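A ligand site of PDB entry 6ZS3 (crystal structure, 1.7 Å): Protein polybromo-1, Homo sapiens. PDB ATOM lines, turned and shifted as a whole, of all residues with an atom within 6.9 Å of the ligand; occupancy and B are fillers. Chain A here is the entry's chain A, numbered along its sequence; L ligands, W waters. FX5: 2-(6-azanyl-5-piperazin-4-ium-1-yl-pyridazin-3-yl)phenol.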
ATOM      1  N   ALA A  40      -6.234  -1.469  36.167  1.00  0.00           N
ATOM      2  CA  ALA A  40      -7.334  -0.564  36.481  1.00  0.00           C
ATOM      3  C   ALA A  40      -7.719   0.356  35.317  1.00  0.00           C
ATOM      4  O   ALA A  40      -8.908   0.495  34.993  1.00  0.00           O
ATOM      5  CB  ALA A  40      -7.003   0.257  37.744  1.00  0.00           C
ATOM      6  N   ILE A  41      -6.738   0.993  34.678  1.00  0.00           N
ATOM      7  CA  ILE A  41      -7.065   1.919  33.589  1.00  0.00           C
ATOM      8  C   ILE A  41      -7.631   1.211  32.366  1.00  0.00           C
ATOM      9  O   ILE A  41      -8.302   1.858  31.553  1.00  0.00           O
ATOM     10  CB  ILE A  41      -5.837   2.771  33.204  1.00  0.00           C
ATOM     11  CG1 ILE A  41      -6.306   4.077  32.563  1.00  0.00           C
ATOM     12  CG2 ILE A  41      -4.869   1.995  32.325  1.00  0.00           C
ATOM     13  CD1 ILE A  41      -6.993   5.037  33.561  1.00  0.00           C
ATOM     14  N   PHE A  42      -7.377  -0.089  32.218  1.00  0.00           N
ATOM     15  CA  PHE A  42      -7.798  -0.829  31.028  1.00  0.00           C
ATOM     16  C   PHE A  42      -9.187  -1.438  31.164  1.00  0.00           C
ATOM     17  O   PHE A  42      -9.650  -2.096  30.231  1.00  0.00           O
ATOM     18  CB  PHE A  42      -6.777  -1.941  30.712  1.00  0.00           C
ATOM     19  CG  PHE A  42      -5.365  -1.413  30.553  1.00  0.00           C
ATOM     20  CD1 PHE A  42      -5.015  -0.636  29.452  1.00  0.00           C
ATOM     21  CD2 PHE A  42      -4.407  -1.673  31.506  1.00  0.00           C
ATOM     22  CE1 PHE A  42      -3.723  -0.134  29.314  1.00  0.00           C
ATOM     23  CE2 PHE A  42      -3.127  -1.172  31.381  1.00  0.00           C
ATOM     24  CZ  PHE A  42      -2.777  -0.385  30.297  1.00  0.00           C
ATOM     25  N   LEU A  43      -9.852  -1.256  32.315  1.00  0.00           N
ATOM     26  CA  LEU A  43     -11.138  -1.942  32.490  1.00  0.00           C
ATOM     27  C   LEU A  43     -12.204  -1.398  31.540  1.00  0.00           C
ATOM     28  O   LEU A  43     -13.043  -2.155  31.046  1.00  0.00           O
ATOM     29  CB  LEU A  43     -11.595  -1.828  33.946  1.00  0.00           C
ATOM     30  CG  LEU A  43     -10.653  -2.491  34.939  1.00  0.00           C
ATOM     31  CD1 LEU A  43     -11.149  -2.244  36.377  1.00  0.00           C
ATOM     32  CD2 LEU A  43     -10.485  -3.966  34.700  1.00  0.00           C
ATOM     33  N   ARG A  44     -12.179  -0.109  31.261  1.00  0.00           N
ATOM     34  CA  ARG A  44     -13.183   0.519  30.420  1.00  0.00           C
ATOM     35  C   ARG A  44     -12.552   1.689  29.665  1.00  0.00           C
ATOM     36  O   ARG A  44     -11.921   2.563  30.277  1.00  0.00           O
ATOM     37  CB  ARG A  44     -14.390   0.962  31.253  1.00  0.00           C
ATOM     38  CG  ARG A  44     -15.409   1.764  30.474  1.00  0.00           C
ATOM     39  CD  ARG A  44     -16.795   1.580  31.058  1.00  0.00           C
ATOM     40  NE  ARG A  44     -17.639   2.756  30.885  1.00  0.00           N
ATOM     41  CZ  ARG A  44     -18.333   3.036  29.789  1.00  0.00           C
ATOM     42  NH1 ARG A  44     -18.282   2.242  28.730  1.00  0.00           N
ATOM     43  NH2 ARG A  44     -19.085   4.126  29.754  1.00  0.00           N
ATOM     44  N   LEU A  45     -12.699   1.681  28.345  1.00  0.00           N
ATOM     45  CA  LEU A  45     -12.185   2.768  27.518  1.00  0.00           C
ATOM     46  C   LEU A  45     -12.891   4.081  27.836  1.00  0.00           C
ATOM     47  O   LEU A  45     -14.072   4.081  28.185  1.00  0.00           O
ATOM     48  CB  LEU A  45     -12.381   2.453  26.043  1.00  0.00           C
ATOM     49  CG  LEU A  45     -11.499   1.450  25.325  1.00  0.00           C
ATOM     50  CD1 LEU A  45     -12.217   0.962  24.075  1.00  0.00           C
ATOM     51  CD2 LEU A  45     -10.184   2.108  24.956  1.00  0.00           C
ATOM     52  N   PRO A  46     -12.202   5.215  27.690  1.00  0.00           N
ATOM     53  CA  PRO A  46     -12.904   6.502  27.606  1.00  0.00           C
ATOM     54  C   PRO A  46     -13.898   6.495  26.452  1.00  0.00           C
ATOM     55  O   PRO A  46     -13.692   5.846  25.427  1.00  0.00           O
ATOM     56  CB  PRO A  46     -11.784   7.507  27.347  1.00  0.00           C
ATOM     57  CG  PRO A  46     -10.541   6.842  27.778  1.00  0.00           C
ATOM     58  CD  PRO A  46     -10.746   5.366  27.562  1.00  0.00           C
ATOM     59  N   GLU A  50     -15.651  11.627  25.229  1.00  0.00           N
ATOM     60  CA  GLU A  50     -14.591  12.023  26.164  1.00  0.00           C
ATOM     61  C   GLU A  50     -13.271  12.274  25.440  1.00  0.00           C
ATOM     62  O   GLU A  50     -12.631  13.313  25.631  1.00  0.00           O
ATOM     63  CB  GLU A  50     -14.458  10.916  27.220  1.00  0.00           C
ATOM     64  CG  GLU A  50     -13.370  11.027  28.273  1.00  0.00           C
ATOM     65  CD  GLU A  50     -13.394   9.837  29.236  1.00  0.00           C
ATOM     66  OE1 GLU A  50     -12.344   9.499  29.823  1.00  0.00           O
ATOM     67  OE2 GLU A  50     -14.468   9.220  29.405  1.00  0.00           O
ATOM     68  N   LEU A  51     -12.859  11.333  24.586  1.00  0.00           N
ATOM     69  CA  LEU A  51     -11.519  11.322  24.014  1.00  0.00           C
ATOM     70  C   LEU A  51     -11.629  10.936  22.541  1.00  0.00           C
ATOM     71  O   LEU A  51     -11.201   9.853  22.116  1.00  0.00           O
ATOM     72  CB  LEU A  51     -10.635  10.335  24.782  1.00  0.00           C
ATOM     73  CG  LEU A  51      -9.109  10.350  24.660  1.00  0.00           C
ATOM     74  CD1 LEU A  51      -8.532  11.653  25.140  1.00  0.00           C
ATOM     75  CD2 LEU A  51      -8.528   9.180  25.459  1.00  0.00           C
ATOM     76  N   TYR A  54      -8.556   9.435  20.477  1.00  0.00           N
ATOM     77  CA  TYR A  54      -8.165   8.040  20.654  1.00  0.00           C
ATOM     78  C   TYR A  54      -8.695   7.199  19.506  1.00  0.00           C
ATOM     79  O   TYR A  54      -7.970   6.368  18.940  1.00  0.00           O
ATOM     80  CB  TYR A  54      -8.702   7.512  22.002  1.00  0.00           C
ATOM     81  CG  TYR A  54      -8.254   6.100  22.336  1.00  0.00           C
ATOM     82  CD1 TYR A  54      -8.951   4.992  21.865  1.00  0.00           C
ATOM     83  CD2 TYR A  54      -7.120   5.879  23.117  1.00  0.00           C
ATOM     84  CE1 TYR A  54      -8.549   3.691  22.183  1.00  0.00           C
ATOM     85  CE2 TYR A  54      -6.704   4.587  23.418  1.00  0.00           C
ATOM     86  CZ  TYR A  54      -7.414   3.511  22.952  1.00  0.00           C
ATOM     87  OH  TYR A  54      -6.960   2.258  23.274  1.00  0.00           O
ATOM     88  N   ILE A  58      -6.859   4.702  16.844  1.00  0.00           N
ATOM     89  CA  ILE A  58      -7.019   3.304  17.217  1.00  0.00           C
ATOM     90  C   ILE A  58      -8.203   2.740  16.445  1.00  0.00           C
ATOM     91  O   ILE A  58      -9.359   3.090  16.727  1.00  0.00           O
ATOM     92  CB  ILE A  58      -7.213   3.152  18.732  1.00  0.00           C
ATOM     93  CG1 ILE A  58      -5.971   3.685  19.461  1.00  0.00           C
ATOM     94  CG2 ILE A  58      -7.564   1.729  19.096  1.00  0.00           C
ATOM     95  CD1 ILE A  58      -4.687   3.001  19.042  1.00  0.00           C
ATOM     96  N   MET A  62     -10.613  -1.750  22.167  1.00  0.00           N
ATOM     97  CA  MET A  62     -10.766  -2.913  23.017  1.00  0.00           C
ATOM     98  C   MET A  62     -10.537  -2.510  24.473  1.00  0.00           C
ATOM     99  O   MET A  62      -9.682  -1.669  24.754  1.00  0.00           O
ATOM    100  CB  MET A  62      -9.786  -4.011  22.603  1.00  0.00           C
ATOM    101  CG  MET A  62      -9.902  -5.318  23.350  1.00  0.00           C
ATOM    102  SD  MET A  62     -11.521  -6.100  23.149  1.00  0.00           S
ATOM    103  CE  MET A  62     -11.728  -6.160  21.375  1.00  0.00           C
ATOM    104  N   ASP A  63     -11.278  -3.126  25.398  1.00  0.00           N
ATOM    105  CA  ASP A  63     -11.000  -2.964  26.817  1.00  0.00           C
ATOM    106  C   ASP A  63     -11.350  -4.267  27.541  1.00  0.00           C
ATOM    107  O   ASP A  63     -11.762  -5.262  26.929  1.00  0.00           O
ATOM    108  CB  ASP A  63     -11.713  -1.724  27.411  1.00  0.00           C
ATOM    109  CG  ASP A  63     -13.228  -1.777  27.253  1.00  0.00           C
ATOM    110  OD1 ASP A  63     -13.799  -2.886  27.158  1.00  0.00           O
ATOM    111  OD2 ASP A  63     -13.840  -0.696  27.250  1.00  0.00           O
ATOM    112  N   MET A  64     -11.162  -4.260  28.859  1.00  0.00           N
ATOM    113  CA  MET A  64     -11.378  -5.511  29.591  1.00  0.00           C
ATOM    114  C   MET A  64     -12.852  -5.788  29.840  1.00  0.00           C
ATOM    115  O   MET A  64     -13.244  -6.957  29.908  1.00  0.00           O
ATOM    116  CB  MET A  64     -10.576  -5.487  30.886  1.00  0.00           C
ATOM    117  CG  MET A  64      -9.076  -5.519  30.572  1.00  0.00           C
ATOM    118  SD  MET A  64      -7.993  -5.696  32.003  1.00  0.00           S
ATOM    119  CE  MET A  64      -8.590  -7.216  32.729  1.00  0.00           C
ATOM    120  N   MET A  89      -5.591  -4.823  22.771  1.00  0.00           N
ATOM    121  CA  MET A  89      -5.812  -3.738  23.716  1.00  0.00           C
ATOM    122  C   MET A  89      -4.489  -3.126  24.173  1.00  0.00           C
ATOM    123  O   MET A  89      -4.338  -1.898  24.212  1.00  0.00           O
ATOM    124  CB  MET A  89      -6.609  -4.287  24.906  1.00  0.00           C
ATOM    125  CG  MET A  89      -6.916  -3.259  25.994  1.00  0.00           C
ATOM    126  SD  MET A  89      -7.631  -4.022  27.468  1.00  0.00           S
ATOM    127  CE  MET A  89      -6.163  -4.669  28.234  1.00  0.00           C
ATOM    128  N   PHE A  90      -3.505  -3.956  24.530  1.00  0.00           N
ATOM    129  CA  PHE A  90      -2.228  -3.413  24.972  1.00  0.00           C
ATOM    130  C   PHE A  90      -1.477  -2.739  23.827  1.00  0.00           C
ATOM    131  O   PHE A  90      -0.856  -1.686  24.033  1.00  0.00           O
ATOM    132  CB  PHE A  90      -1.371  -4.518  25.589  1.00  0.00           C
ATOM    133  CG  PHE A  90      -1.937  -5.108  26.860  1.00  0.00           C
ATOM    134  CD1 PHE A  90      -2.389  -4.280  27.888  1.00  0.00           C
ATOM    135  CD2 PHE A  90      -2.031  -6.470  27.024  1.00  0.00           C
ATOM    136  CE1 PHE A  90      -2.910  -4.804  29.048  1.00  0.00           C
ATOM    137  CE2 PHE A  90      -2.561  -7.023  28.213  1.00  0.00           C
ATOM    138  CZ  PHE A  90      -3.008  -6.181  29.208  1.00  0.00           C
ATOM    139  N   ASN A  92      -2.962  -1.223  21.383  1.00  0.00           N
ATOM    140  CA  ASN A  92      -3.672   0.052  21.237  1.00  0.00           C
ATOM    141  C   ASN A  92      -3.170   1.084  22.251  1.00  0.00           C
ATOM    142  O   ASN A  92      -2.904   2.232  21.890  1.00  0.00           O
ATOM    143  CB  ASN A  92      -5.180  -0.129  21.409  1.00  0.00           C
ATOM    144  CG  ASN A  92      -5.843  -0.884  20.242  1.00  0.00           C
ATOM    145  OD1 ASN A  92      -5.292  -1.008  19.134  1.00  0.00           O
ATOM    146  ND2 ASN A  92      -7.062  -1.347  20.480  1.00  0.00           N
ATOM    147  N   ALA A  93      -3.084   0.684  23.523  1.00  0.00           N
ATOM    148  CA  ALA A  93      -2.594   1.578  24.561  1.00  0.00           C
ATOM    149  C   ALA A  93      -1.200   2.103  24.229  1.00  0.00           C
ATOM    150  O   ALA A  93      -0.906   3.290  24.424  1.00  0.00           O
ATOM    151  CB  ALA A  93      -2.597   0.868  25.915  1.00  0.00           C
ATOM    152  N   CYS A  94      -0.329   1.243  23.683  1.00  0.00           N
ATOM    153  CA  CYS A  94       1.035   1.650  23.399  1.00  0.00           C
ATOM    154  C   CYS A  94       1.156   2.389  22.068  1.00  0.00           C
ATOM    155  O   CYS A  94       2.191   3.039  21.836  1.00  0.00           O
ATOM    156  CB  CYS A  94       1.962   0.432  23.441  1.00  0.00           C
ATOM    157  SG  CYS A  94       2.171  -0.183  25.133  1.00  0.00           S
ATOM    158  N   TYR A  96      -1.363   4.724  21.225  1.00  0.00           N
ATOM    159  CA  TYR A  96      -1.910   6.024  21.576  1.00  0.00           C
ATOM    160  C   TYR A  96      -1.000   6.798  22.531  1.00  0.00           C
ATOM    161  O   TYR A  96      -0.858   8.023  22.399  1.00  0.00           O
ATOM    162  CB  TYR A  96      -3.294   5.860  22.195  1.00  0.00           C
ATOM    163  CG  TYR A  96      -3.936   7.172  22.603  1.00  0.00           C
ATOM    164  CD1 TYR A  96      -4.455   8.023  21.638  1.00  0.00           C
ATOM    165  CD2 TYR A  96      -4.046   7.542  23.947  1.00  0.00           C
ATOM    166  CE1 TYR A  96      -5.042   9.246  22.003  1.00  0.00           C
ATOM    167  CE2 TYR A  96      -4.637   8.744  24.312  1.00  0.00           C
ATOM    168  CZ  TYR A  96      -5.136   9.593  23.336  1.00  0.00           C
ATOM    169  OH  TYR A  96      -5.718  10.787  23.694  1.00  0.00           O
ATOM    170  N   ASN A  97      -0.396   6.136  23.508  1.00  0.00           N
ATOM    171  CA  ASN A  97       0.413   6.799  24.511  1.00  0.00           C
ATOM    172  C   ASN A  97       1.892   6.749  24.140  1.00  0.00           C
ATOM    173  O   ASN A  97       2.331   5.869  23.399  1.00  0.00           O
ATOM    174  CB  ASN A  97       0.211   6.171  25.887  1.00  0.00           C
ATOM    175  CG  ASN A  97      -1.242   6.234  26.354  1.00  0.00           C
ATOM    176  OD1 ASN A  97      -1.680   7.260  26.859  1.00  0.00           O
ATOM    177  ND2 ASN A  97      -1.982   5.134  26.193  1.00  0.00           N
ATOM    178  N   ILE A 103       0.858   4.645  31.401  1.00  0.00           N
ATOM    179  CA  ILE A 103      -0.076   3.675  30.828  1.00  0.00           C
ATOM    180  C   ILE A 103       0.634   2.775  29.839  1.00  0.00           C
ATOM    181  O   ILE A 103       0.396   1.561  29.785  1.00  0.00           O
ATOM    182  CB  ILE A 103      -1.274   4.418  30.187  1.00  0.00           C
ATOM    183  CG1 ILE A 103      -2.132   5.075  31.280  1.00  0.00           C
ATOM    184  CG2 ILE A 103      -2.090   3.467  29.341  1.00  0.00           C
ATOM    185  CD1 ILE A 103      -3.115   6.127  30.794  1.00  0.00           C
HETATM  186  C4  FX5 L   1      -8.188   2.358  28.263  1.00  0.00           C
HETATM  187  C5  FX5 L   1      -7.158   2.781  27.410  1.00  0.00           C
HETATM  188  C6  FX5 L   1      -6.697   1.876  26.438  1.00  0.00           C
HETATM  189  C7  FX5 L   1      -6.555   4.135  27.569  1.00  0.00           C
HETATM  190  C8  FX5 L   1      -7.044   5.075  28.487  1.00  0.00           C
HETATM  191  C10 FX5 L   1      -5.244   6.502  27.768  1.00  0.00           C
HETATM  192  N12 FX5 L   1      -5.497   4.395  26.798  1.00  0.00           N
HETATM  193  C17 FX5 L   1      -7.784   8.154  31.510  1.00  0.00           C
HETATM  194  C20 FX5 L   1      -7.143   8.628  28.784  1.00  0.00           C
HETATM  195  C1  FX5 L   1      -7.245   0.600  26.335  1.00  0.00           C
HETATM  196  C16 FX5 L   1      -7.789   7.043  30.478  1.00  0.00           C
HETATM  197  C19 FX5 L   1      -7.114   9.746  29.799  1.00  0.00           C
HETATM  198  C2  FX5 L   1      -8.257   0.215  27.199  1.00  0.00           C
HETATM  199  C3  FX5 L   1      -8.724   1.088  28.155  1.00  0.00           C
HETATM  200  C9  FX5 L   1      -6.386   6.297  28.592  1.00  0.00           C
HETATM  201  N11 FX5 L   1      -4.839   5.566  26.898  1.00  0.00           N
HETATM  202  N14 FX5 L   1      -4.461   7.586  27.842  1.00  0.00           N
HETATM  203  N15 FX5 L   1      -6.811   7.356  29.437  1.00  0.00           N
HETATM  204  N18 FX5 L   1      -8.070   9.453  30.884  1.00  0.00           N
HETATM  205  O13 FX5 L   1      -5.731   2.233  25.546  1.00  0.00           O
HETATM  206  O   HOH W   1      -3.550   9.547  29.994  1.00  0.00           O
HETATM  207  O   HOH W   2      -9.705   3.980  30.814  1.00  0.00           O
HETATM  208  O   HOH W   3      -7.306  12.885  28.325  1.00  0.00           O
HETATM  209  O   HOH W   4     -10.325   6.266  32.554  1.00  0.00           O
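The side-chain hydroxyl (OH) of Tyr 54 lies within hydrogen-bond range of an oxygen (O13) of the ligand, 2.6 Å away. N14 of the ligand lies within hydrogen-bond range of OD1 of Asn 97 (3.0 Å).
The side-chain amide nitrogen of Asn 97 lies within hydrogen-bond range of the backbone carbonyl oxygen of Ala 93. The backbone NH (N) of Leu 45 sits at hydrogen-bond distance from the side-chain carboxylate (OD2) of Asp 63 (2.9 Å). The backbone carbonyl oxygen (O) of Phe 42 lies within hydrogen-bond range of the backbone NH (N) of Met 64, at 3.0 Å.
Residues that only touch the ligand: Ile 41 (3.3 Å), Phe 42 (3.6 Å), Leu 45 (3.5 Å), Pro 46 (3.8 Å), Leu 51 (3.6 Å), Met 62 (3.4 Å), Asp 63 (3.97 Å), Met 89 (3.9 Å), Ala 93 (3.4 Å), Tyr 96 (3.6 Å) and Ile 103 (3.6 Å). The nearest printed residue that does not touch the ligand is Arg 44 (4.1 Å).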
